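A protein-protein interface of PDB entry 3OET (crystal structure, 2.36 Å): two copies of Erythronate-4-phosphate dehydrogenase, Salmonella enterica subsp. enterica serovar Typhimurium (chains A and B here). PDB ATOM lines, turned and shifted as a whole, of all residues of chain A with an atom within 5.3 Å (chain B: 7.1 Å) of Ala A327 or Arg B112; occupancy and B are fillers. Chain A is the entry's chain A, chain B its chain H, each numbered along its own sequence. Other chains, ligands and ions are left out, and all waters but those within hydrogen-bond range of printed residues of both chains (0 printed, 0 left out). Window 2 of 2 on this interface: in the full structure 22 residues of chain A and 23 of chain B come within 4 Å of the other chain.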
ATOM      1  N   ARG A 323     -36.019  32.841  -4.773  1.00  0.00           N
ATOM      2  CA  ARG A 323     -35.041  31.740  -4.751  1.00  0.00           C
ATOM      3  C   ARG A 323     -33.637  32.148  -4.383  1.00  0.00           C
ATOM      4  O   ARG A 323     -32.838  31.307  -3.937  1.00  0.00           O
ATOM      5  CB  ARG A 323     -35.050  30.982  -6.076  1.00  0.00           C
ATOM      6  CG  ARG A 323     -36.292  30.131  -6.182  1.00  0.00           C
ATOM      7  CD  ARG A 323     -36.498  29.545  -7.539  1.00  0.00           C
ATOM      8  NE  ARG A 323     -36.670  30.602  -8.515  1.00  0.00           N
ATOM      9  CZ  ARG A 323     -36.923  30.387  -9.799  1.00  0.00           C
ATOM     10  NH1 ARG A 323     -37.051  29.130 -10.246  1.00  0.00           N
ATOM     11  NH2 ARG A 323     -37.054  31.433 -10.621  1.00  0.00           N
ATOM     12  N   ARG A 324     -33.310  33.432  -4.553  1.00  0.00           N
ATOM     13  CA  ARG A 324     -31.984  33.873  -4.143  1.00  0.00           C
ATOM     14  C   ARG A 324     -31.795  33.861  -2.615  1.00  0.00           C
ATOM     15  O   ARG A 324     -30.678  33.800  -2.155  1.00  0.00           O
ATOM     16  CB  ARG A 324     -31.621  35.233  -4.718  1.00  0.00           C
ATOM     17  CG  ARG A 324     -31.952  36.379  -3.827  1.00  0.00           C
ATOM     18  CD  ARG A 324     -30.737  37.253  -3.664  1.00  0.00           C
ATOM     19  NE  ARG A 324     -31.048  38.685  -3.792  1.00  0.00           N
ATOM     20  CZ  ARG A 324     -31.326  39.496  -2.772  1.00  0.00           C
ATOM     21  NH1 ARG A 324     -31.378  39.015  -1.544  1.00  0.00           N
ATOM     22  NH2 ARG A 324     -31.578  40.782  -2.990  1.00  0.00           N
ATOM     23  N   ASP A 325     -32.881  33.938  -1.842  1.00  0.00           N
ATOM     24  CA  ASP A 325     -32.764  33.830  -0.379  1.00  0.00           C
ATOM     25  C   ASP A 325     -33.016  32.376   0.135  1.00  0.00           C
ATOM     26  O   ASP A 325     -32.533  32.021   1.187  1.00  0.00           O
ATOM     27  CB  ASP A 325     -33.666  34.847   0.353  1.00  0.00           C
ATOM     28  CG  ASP A 325     -33.391  36.305  -0.066  1.00  0.00           C
ATOM     29  OD1 ASP A 325     -32.225  36.698  -0.255  1.00  0.00           O
ATOM     30  OD2 ASP A 325     -34.351  37.071  -0.208  1.00  0.00           O
ATOM     31  N   ASP A 326     -33.783  31.575  -0.618  1.00  0.00           N
ATOM     32  CA  ASP A 326     -34.036  30.183  -0.302  1.00  0.00           C
ATOM     33  C   ASP A 326     -32.750  29.374  -0.371  1.00  0.00           C
ATOM     34  O   ASP A 326     -32.444  28.596   0.528  1.00  0.00           O
ATOM     35  CB  ASP A 326     -35.080  29.575  -1.266  1.00  0.00           C
ATOM     36  CG  ASP A 326     -35.263  28.058  -1.068  1.00  0.00           C
ATOM     37  OD1 ASP A 326     -36.321  27.613  -0.547  1.00  0.00           O
ATOM     38  OD2 ASP A 326     -34.347  27.301  -1.416  1.00  0.00           O
ATOM     39  N   ALA A 327     -31.999  29.557  -1.451  1.00  0.00           N
ATOM     40  CA  ALA A 327     -30.832  28.711  -1.687  1.00  0.00           C
ATOM     41  C   ALA A 327     -29.763  28.802  -0.597  1.00  0.00           C
ATOM     42  O   ALA A 327     -29.267  27.774  -0.157  1.00  0.00           O
ATOM     43  CB  ALA A 327     -30.241  28.974  -3.072  1.00  0.00           C
ATOM     44  N   PRO A 328     -29.408  30.024  -0.153  1.00  0.00           N
ATOM     45  CA  PRO A 328     -28.375  30.101   0.907  1.00  0.00           C
ATOM     46  C   PRO A 328     -28.843  29.609   2.271  1.00  0.00           C
ATOM     47  O   PRO A 328     -28.020  29.209   3.095  1.00  0.00           O
ATOM     48  CB  PRO A 328     -28.011  31.603   0.967  1.00  0.00           C
ATOM     49  CG  PRO A 328     -29.188  32.339   0.288  1.00  0.00           C
ATOM     50  CD  PRO A 328     -29.668  31.343  -0.777  1.00  0.00           C
ATOM     51  N   LEU A 329     -30.150  29.619   2.514  1.00  0.00           N
ATOM     52  CA  LEU A 329     -30.645  29.099   3.763  1.00  0.00           C
ATOM     53  C   LEU A 329     -30.530  27.571   3.745  1.00  0.00           C
ATOM     54  O   LEU A 329     -30.199  26.955   4.768  1.00  0.00           O
ATOM     55  CB  LEU A 329     -32.086  29.555   4.059  1.00  0.00           C
ATOM     56  CG  LEU A 329     -32.642  28.945   5.359  1.00  0.00           C
ATOM     57  CD1 LEU A 329     -31.706  29.271   6.532  1.00  0.00           C
ATOM     58  CD2 LEU A 329     -34.086  29.382   5.671  1.00  0.00           C
ATOM     59  N   ARG A 330     -30.774  26.946   2.590  1.00  0.00           N
ATOM     60  CA  ARG A 330     -30.637  25.486   2.539  1.00  0.00           C
ATOM     61  C   ARG A 330     -29.180  25.078   2.739  1.00  0.00           C
ATOM     62  O   ARG A 330     -28.887  24.014   3.262  1.00  0.00           O
ATOM     63  CB  ARG A 330     -31.155  24.927   1.227  1.00  0.00           C
ATOM     64  CG  ARG A 330     -32.653  24.997   1.109  1.00  0.00           C
ATOM     65  CD  ARG A 330     -33.128  24.357  -0.155  1.00  0.00           C
ATOM     66  NE  ARG A 330     -34.451  24.863  -0.468  1.00  0.00           N
ATOM     67  CZ  ARG A 330     -35.580  24.341  -0.018  1.00  0.00           C
ATOM     68  NH1 ARG A 330     -35.545  23.260   0.751  1.00  0.00           N
ATOM     69  NH2 ARG A 330     -36.750  24.888  -0.356  1.00  0.00           N
ATOM     70  N   LYS A 331     -28.255  25.933   2.328  1.00  0.00           N
ATOM     71  CA  LYS A 331     -26.844  25.562   2.405  1.00  0.00           C
ATOM     72  C   LYS A 331     -26.327  25.533   3.852  1.00  0.00           C
ATOM     73  O   LYS A 331     -25.388  24.822   4.143  1.00  0.00           O
ATOM     74  CB  LYS A 331     -26.010  26.508   1.547  1.00  0.00           C
ATOM     75  CG  LYS A 331     -24.699  25.917   1.057  1.00  0.00           C
ATOM     76  CD  LYS A 331     -23.724  27.007   0.573  1.00  0.00           C
ATOM     77  CE  LYS A 331     -22.388  26.401   0.087  1.00  0.00           C
ATOM     78  NZ  LYS A 331     -21.313  27.423  -0.033  1.00  0.00           N
ATOM     79  N   LEU B 106     -25.430  27.691 -15.885  1.00  0.00           N
ATOM     80  CA  LEU B 106     -24.315  27.985 -14.973  1.00  0.00           C
ATOM     81  C   LEU B 106     -24.597  29.121 -13.981  1.00  0.00           C
ATOM     82  O   LEU B 106     -24.116  29.093 -12.847  1.00  0.00           O
ATOM     83  CB  LEU B 106     -23.061  28.364 -15.760  1.00  0.00           C
ATOM     84  CG  LEU B 106     -22.229  27.261 -16.401  1.00  0.00           C
ATOM     85  CD1 LEU B 106     -21.313  27.856 -17.441  1.00  0.00           C
ATOM     86  CD2 LEU B 106     -21.452  26.530 -15.321  1.00  0.00           C
ATOM     87  N   LEU B 107     -25.298  30.146 -14.454  1.00  0.00           N
ATOM     88  CA  LEU B 107     -25.674  31.272 -13.614  1.00  0.00           C
ATOM     89  C   LEU B 107     -26.712  30.821 -12.591  1.00  0.00           C
ATOM     90  O   LEU B 107     -26.659  31.229 -11.438  1.00  0.00           O
ATOM     91  CB  LEU B 107     -26.175  32.460 -14.455  1.00  0.00           C
ATOM     92  CG  LEU B 107     -25.091  33.242 -15.207  1.00  0.00           C
ATOM     93  CD1 LEU B 107     -25.656  34.119 -16.318  1.00  0.00           C
ATOM     94  CD2 LEU B 107     -24.258  34.106 -14.232  1.00  0.00           C
ATOM     95  N   MET B 108     -27.618  29.934 -12.992  1.00  0.00           N
ATOM     96  CA  MET B 108     -28.541  29.337 -12.029  1.00  0.00           C
ATOM     97  C   MET B 108     -27.790  28.502 -10.949  1.00  0.00           C
ATOM     98  O   MET B 108     -28.099  28.567  -9.766  1.00  0.00           O
ATOM     99  CB  MET B 108     -29.609  28.510 -12.746  1.00  0.00           C
ATOM    100  CG  MET B 108     -30.661  27.912 -11.838  1.00  0.00           C
ATOM    101  SD  MET B 108     -30.044  26.236 -10.985  1.00  0.00           S
ATOM    102  CE  MET B 108     -31.674  25.634 -10.035  1.00  0.00           C
ATOM    103  N   LEU B 109     -26.796  27.733 -11.357  1.00  0.00           N
ATOM    104  CA  LEU B 109     -26.105  26.875 -10.411  1.00  0.00           C
ATOM    105  C   LEU B 109     -25.203  27.696  -9.482  1.00  0.00           C
ATOM    106  O   LEU B 109     -25.141  27.427  -8.272  1.00  0.00           O
ATOM    107  CB  LEU B 109     -25.353  25.762 -11.157  1.00  0.00           C
ATOM    108  CG  LEU B 109     -26.252  24.649 -11.748  1.00  0.00           C
ATOM    109  CD1 LEU B 109     -25.659  24.055 -12.977  1.00  0.00           C
ATOM    110  CD2 LEU B 109     -26.554  23.557 -10.730  1.00  0.00           C
ATOM    111  N   ALA B 110     -24.542  28.717 -10.033  1.00  0.00           N
ATOM    112  CA  ALA B 110     -23.687  29.589  -9.235  1.00  0.00           C
ATOM    113  C   ALA B 110     -24.448  30.289  -8.107  1.00  0.00           C
ATOM    114  O   ALA B 110     -23.892  30.474  -7.018  1.00  0.00           O
ATOM    115  CB  ALA B 110     -22.997  30.612 -10.110  1.00  0.00           C
ATOM    116  N   GLU B 111     -25.705  30.687  -8.373  1.00  0.00           N
ATOM    117  CA  GLU B 111     -26.576  31.269  -7.340  1.00  0.00           C
ATOM    118  C   GLU B 111     -27.060  30.215  -6.372  1.00  0.00           C
ATOM    119  O   GLU B 111     -26.959  30.372  -5.154  1.00  0.00           O
ATOM    120  CB  GLU B 111     -27.796  31.954  -7.938  1.00  0.00           C
ATOM    121  CG  GLU B 111     -28.757  32.481  -6.864  1.00  0.00           C
ATOM    122  CD  GLU B 111     -30.047  33.074  -7.455  1.00  0.00           C
ATOM    123  OE1 GLU B 111     -30.939  32.301  -7.879  1.00  0.00           O
ATOM    124  OE2 GLU B 111     -30.166  34.316  -7.488  1.00  0.00           O
ATOM    125  N   ARG B 112     -27.597  29.134  -6.915  1.00  0.00           N
ATOM    126  CA  ARG B 112     -28.070  28.070  -6.059  1.00  0.00           C
ATOM    127  C   ARG B 112     -26.980  27.640  -5.055  1.00  0.00           C
ATOM    128  O   ARG B 112     -27.229  27.606  -3.847  1.00  0.00           O
ATOM    129  CB  ARG B 112     -28.545  26.891  -6.893  1.00  0.00           C
ATOM    130  CG  ARG B 112     -29.531  25.977  -6.157  1.00  0.00           C
ATOM    131  CD  ARG B 112     -29.664  24.645  -6.861  1.00  0.00           C
ATOM    132  NE  ARG B 112     -28.401  23.923  -6.787  1.00  0.00           N
ATOM    133  CZ  ARG B 112     -28.126  22.804  -7.444  1.00  0.00           C
ATOM    134  NH1 ARG B 112     -29.027  22.262  -8.262  1.00  0.00           N
ATOM    135  NH2 ARG B 112     -26.939  22.239  -7.290  1.00  0.00           N
ATOM    136  N   ASP B 113     -25.775  27.356  -5.554  1.00  0.00           N
ATOM    137  CA  ASP B 113     -24.693  26.828  -4.724  1.00  0.00           C
ATOM    138  C   ASP B 113     -23.710  27.853  -4.125  1.00  0.00           C
ATOM    139  O   ASP B 113     -22.854  27.503  -3.319  1.00  0.00           O
ATOM    140  CB  ASP B 113     -23.961  25.713  -5.477  1.00  0.00           C
ATOM    141  CG  ASP B 113     -24.884  24.572  -5.825  1.00  0.00           C
ATOM    142  OD1 ASP B 113     -25.927  24.443  -5.160  1.00  0.00           O
ATOM    143  OD2 ASP B 113     -24.593  23.808  -6.755  1.00  0.00           O
ATOM    144  N   GLY B 114     -23.858  29.118  -4.497  1.00  0.00           N
ATOM    145  CA  GLY B 114     -23.095  30.179  -3.867  1.00  0.00           C
ATOM    146  C   GLY B 114     -21.623  30.174  -4.243  1.00  0.00           C
ATOM    147  O   GLY B 114     -20.773  30.456  -3.396  1.00  0.00           O
ATOM    148  N   PHE B 115     -21.298  29.865  -5.503  1.00  0.00           N
ATOM    149  CA  PHE B 115     -19.914  30.040  -5.938  1.00  0.00           C
ATOM    150  C   PHE B 115     -19.801  31.188  -6.915  1.00  0.00           C
ATOM    151  O   PHE B 115     -20.795  31.622  -7.463  1.00  0.00           O
ATOM    152  CB  PHE B 115     -19.295  28.750  -6.499  1.00  0.00           C
ATOM    153  CG  PHE B 115     -20.037  28.161  -7.677  1.00  0.00           C
ATOM    154  CD1 PHE B 115     -19.826  28.638  -8.966  1.00  0.00           C
ATOM    155  CD2 PHE B 115     -20.922  27.109  -7.497  1.00  0.00           C
ATOM    156  CE1 PHE B 115     -20.506  28.085 -10.046  1.00  0.00           C
ATOM    157  CE2 PHE B 115     -21.590  26.556  -8.560  1.00  0.00           C
ATOM    158  CZ  PHE B 115     -21.381  27.044  -9.839  1.00  0.00           C
ATOM    159  N   LEU B 230     -21.684  15.462  -7.913  1.00  0.00           N
ATOM    160  CA  LEU B 230     -21.589  15.970  -9.245  1.00  0.00           C
ATOM    161  C   LEU B 230     -22.878  16.740  -9.583  1.00  0.00           C
ATOM    162  O   LEU B 230     -23.975  16.438  -9.072  1.00  0.00           O
ATOM    163  CB  LEU B 230     -21.327  14.814 -10.213  1.00  0.00           C
ATOM    164  CG  LEU B 230     -21.040  15.077 -11.699  1.00  0.00           C
ATOM    165  CD1 LEU B 230     -19.656  15.680 -11.960  1.00  0.00           C
ATOM    166  CD2 LEU B 230     -21.218  13.784 -12.471  1.00  0.00           C
ATOM    167  N   SER B 231     -22.730  17.760 -10.417  1.00  0.00           N
ATOM    168  CA  SER B 231     -23.868  18.489 -10.911  1.00  0.00           C
ATOM    169  C   SER B 231     -23.978  18.199 -12.394  1.00  0.00           C
ATOM    170  O   SER B 231     -22.965  18.093 -13.097  1.00  0.00           O
ATOM    171  CB  SER B 231     -23.706  19.987 -10.651  1.00  0.00           C
ATOM    172  OG  SER B 231     -23.995  20.300  -9.293  1.00  0.00           O
ATOM    173  N   VAL B 251     -30.418  14.630 -12.505  1.00  0.00           N
ATOM    174  CA  VAL B 251     -29.691  15.787 -13.014  1.00  0.00           C
ATOM    175  C   VAL B 251     -30.199  17.068 -12.359  1.00  0.00           C
ATOM    176  O   VAL B 251     -31.309  17.101 -11.818  1.00  0.00           O
ATOM    177  CB  VAL B 251     -29.815  15.916 -14.541  1.00  0.00           C
ATOM    178  CG1 VAL B 251     -29.245  14.658 -15.238  1.00  0.00           C
ATOM    179  CG2 VAL B 251     -31.279  16.200 -14.953  1.00  0.00           C
ATOM    180  N   ASP B 252     -29.377  18.111 -12.394  1.00  0.00           N
ATOM    181  CA  ASP B 252     -29.775  19.420 -11.867  1.00  0.00           C
ATOM    182  C   ASP B 252     -30.658  20.174 -12.846  1.00  0.00           C
ATOM    183  O   ASP B 252     -31.564  20.884 -12.427  1.00  0.00           O
ATOM    184  CB  ASP B 252     -28.551  20.274 -11.523  1.00  0.00           C
ATOM    185  CG  ASP B 252     -27.785  19.747 -10.315  1.00  0.00           C
ATOM    186  OD1 ASP B 252     -27.998  20.295  -9.208  1.00  0.00           O
ATOM    187  OD2 ASP B 252     -26.961  18.798 -10.464  1.00  0.00           O
ATOM    188  N   ILE B 253     -30.376  20.045 -14.141  1.00  0.00           N
ATOM    189  CA  ILE B 253     -31.219  20.635 -15.169  1.00  0.00           C
ATOM    190  C   ILE B 253     -31.299  19.647 -16.310  1.00  0.00           C
ATOM    191  O   ILE B 253     -30.256  19.134 -16.791  1.00  0.00           O
ATOM    192  CB  ILE B 253     -30.604  21.907 -15.796  1.00  0.00           C
ATOM    193  CG1 ILE B 253     -30.583  23.101 -14.830  1.00  0.00           C
ATOM    194  CG2 ILE B 253     -31.344  22.268 -17.094  1.00  0.00           C
ATOM    195  CD1 ILE B 253     -31.941  23.706 -14.664  1.00  0.00           C
ATOM    196  N   LYS B 313     -26.618  37.734 -13.947  1.00  0.00           N
ATOM    197  CA  LYS B 313     -27.607  36.656 -13.889  1.00  0.00           C
ATOM    198  C   LYS B 313     -28.983  37.247 -14.145  1.00  0.00           C
ATOM    199  O   LYS B 313     -29.803  36.679 -14.877  1.00  0.00           O
ATOM    200  CB  LYS B 313     -27.617  35.933 -12.543  1.00  0.00           C
ATOM    201  CG  LYS B 313     -28.764  34.935 -12.443  1.00  0.00           C
ATOM    202  CD  LYS B 313     -28.809  34.220 -11.083  1.00  0.00           C
ATOM    203  CE  LYS B 313     -30.051  33.322 -10.959  1.00  0.00           C
ATOM    204  NZ  LYS B 313     -31.373  34.031 -11.130  1.00  0.00           N
ATOM    205  N   ARG B 323     -34.688  27.360 -16.418  1.00  0.00           N
ATOM    206  CA  ARG B 323     -35.584  26.632 -15.517  1.00  0.00           C
ATOM    207  C   ARG B 323     -36.991  26.548 -16.056  1.00  0.00           C
ATOM    208  O   ARG B 323     -37.769  25.663 -15.662  1.00  0.00           O
ATOM    209  CB  ARG B 323     -35.603  27.254 -14.128  1.00  0.00           C
ATOM    210  CG  ARG B 323     -34.481  26.761 -13.215  1.00  0.00           C
ATOM    211  CD  ARG B 323     -34.416  27.624 -11.981  1.00  0.00           C
ATOM    212  NE  ARG B 323     -34.116  28.990 -12.372  1.00  0.00           N
ATOM    213  CZ  ARG B 323     -33.740  29.947 -11.534  1.00  0.00           C
ATOM    214  NH1 ARG B 323     -33.616  29.695 -10.232  1.00  0.00           N
ATOM    215  NH2 ARG B 323     -33.514  31.161 -12.002  1.00  0.00           N
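The guanidinium group (NH1) of Arg B323 sits close to the guanidinium group (NH1) of Arg A323 (3.5 Å).
Among the printed residues, pairs that only touch across the chains: Arg A324 with Glu B111, Ala A327 with Arg B112 and Lys A331 with Asp B113.
Of the printed residues of chain B, Ala A327 touches Arg B112 (3.4 Å).
Printed residues of chain A within 4 Å of Arg B112: Ala A327.
Printed residues of chain A within 4 Å of Glu B111: Arg A324.
Of the printed residues of chain B, Arg A324 touches Glu B111.
Printed residues of chain B within 4 Å of Lys A331: Asp B113.
The guanidinium group (NH1) of Arg A324 lies within salt-bridge range of the side-chain carboxylate (OD1) of Asp A325, 2.8 Å away.
The side-chain carboxylate (OD2) of Asp B113 is in salt-bridge range of the guanidinium group (NH2) of Arg B112, at 2.9 Å.
OE1 of Glu B111 is in salt-bridge range of NZ of Lys B313 (3.7 Å).
The guanidinium group of Arg B112 is in salt-bridge range of the side-chain carboxylate of Asp B252 (2.4 Å).
Arg B323 touches its own counterpart, Arg A323.
Of the 4 pairs that touch across the chains among the printed residues, 1 has its exchanged pair printed and touching as well.
Of the 17 printed residues of chain B, 4 touch a printed residue of chain A.
Of the 9 printed residues of chain A, 4 touch a printed residue of chain B.
Hydrophobic or aromatic side chains of chain A that line the printed part of chain B: Ala A327.
Along chain A the printed residues that touch a printed residue of chain B span positions 323 to 331.
Among the printed residues, no Asp or Glu carboxylate lies within 4 Å of a Lys or Arg side-chain nitrogen of the other chain.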
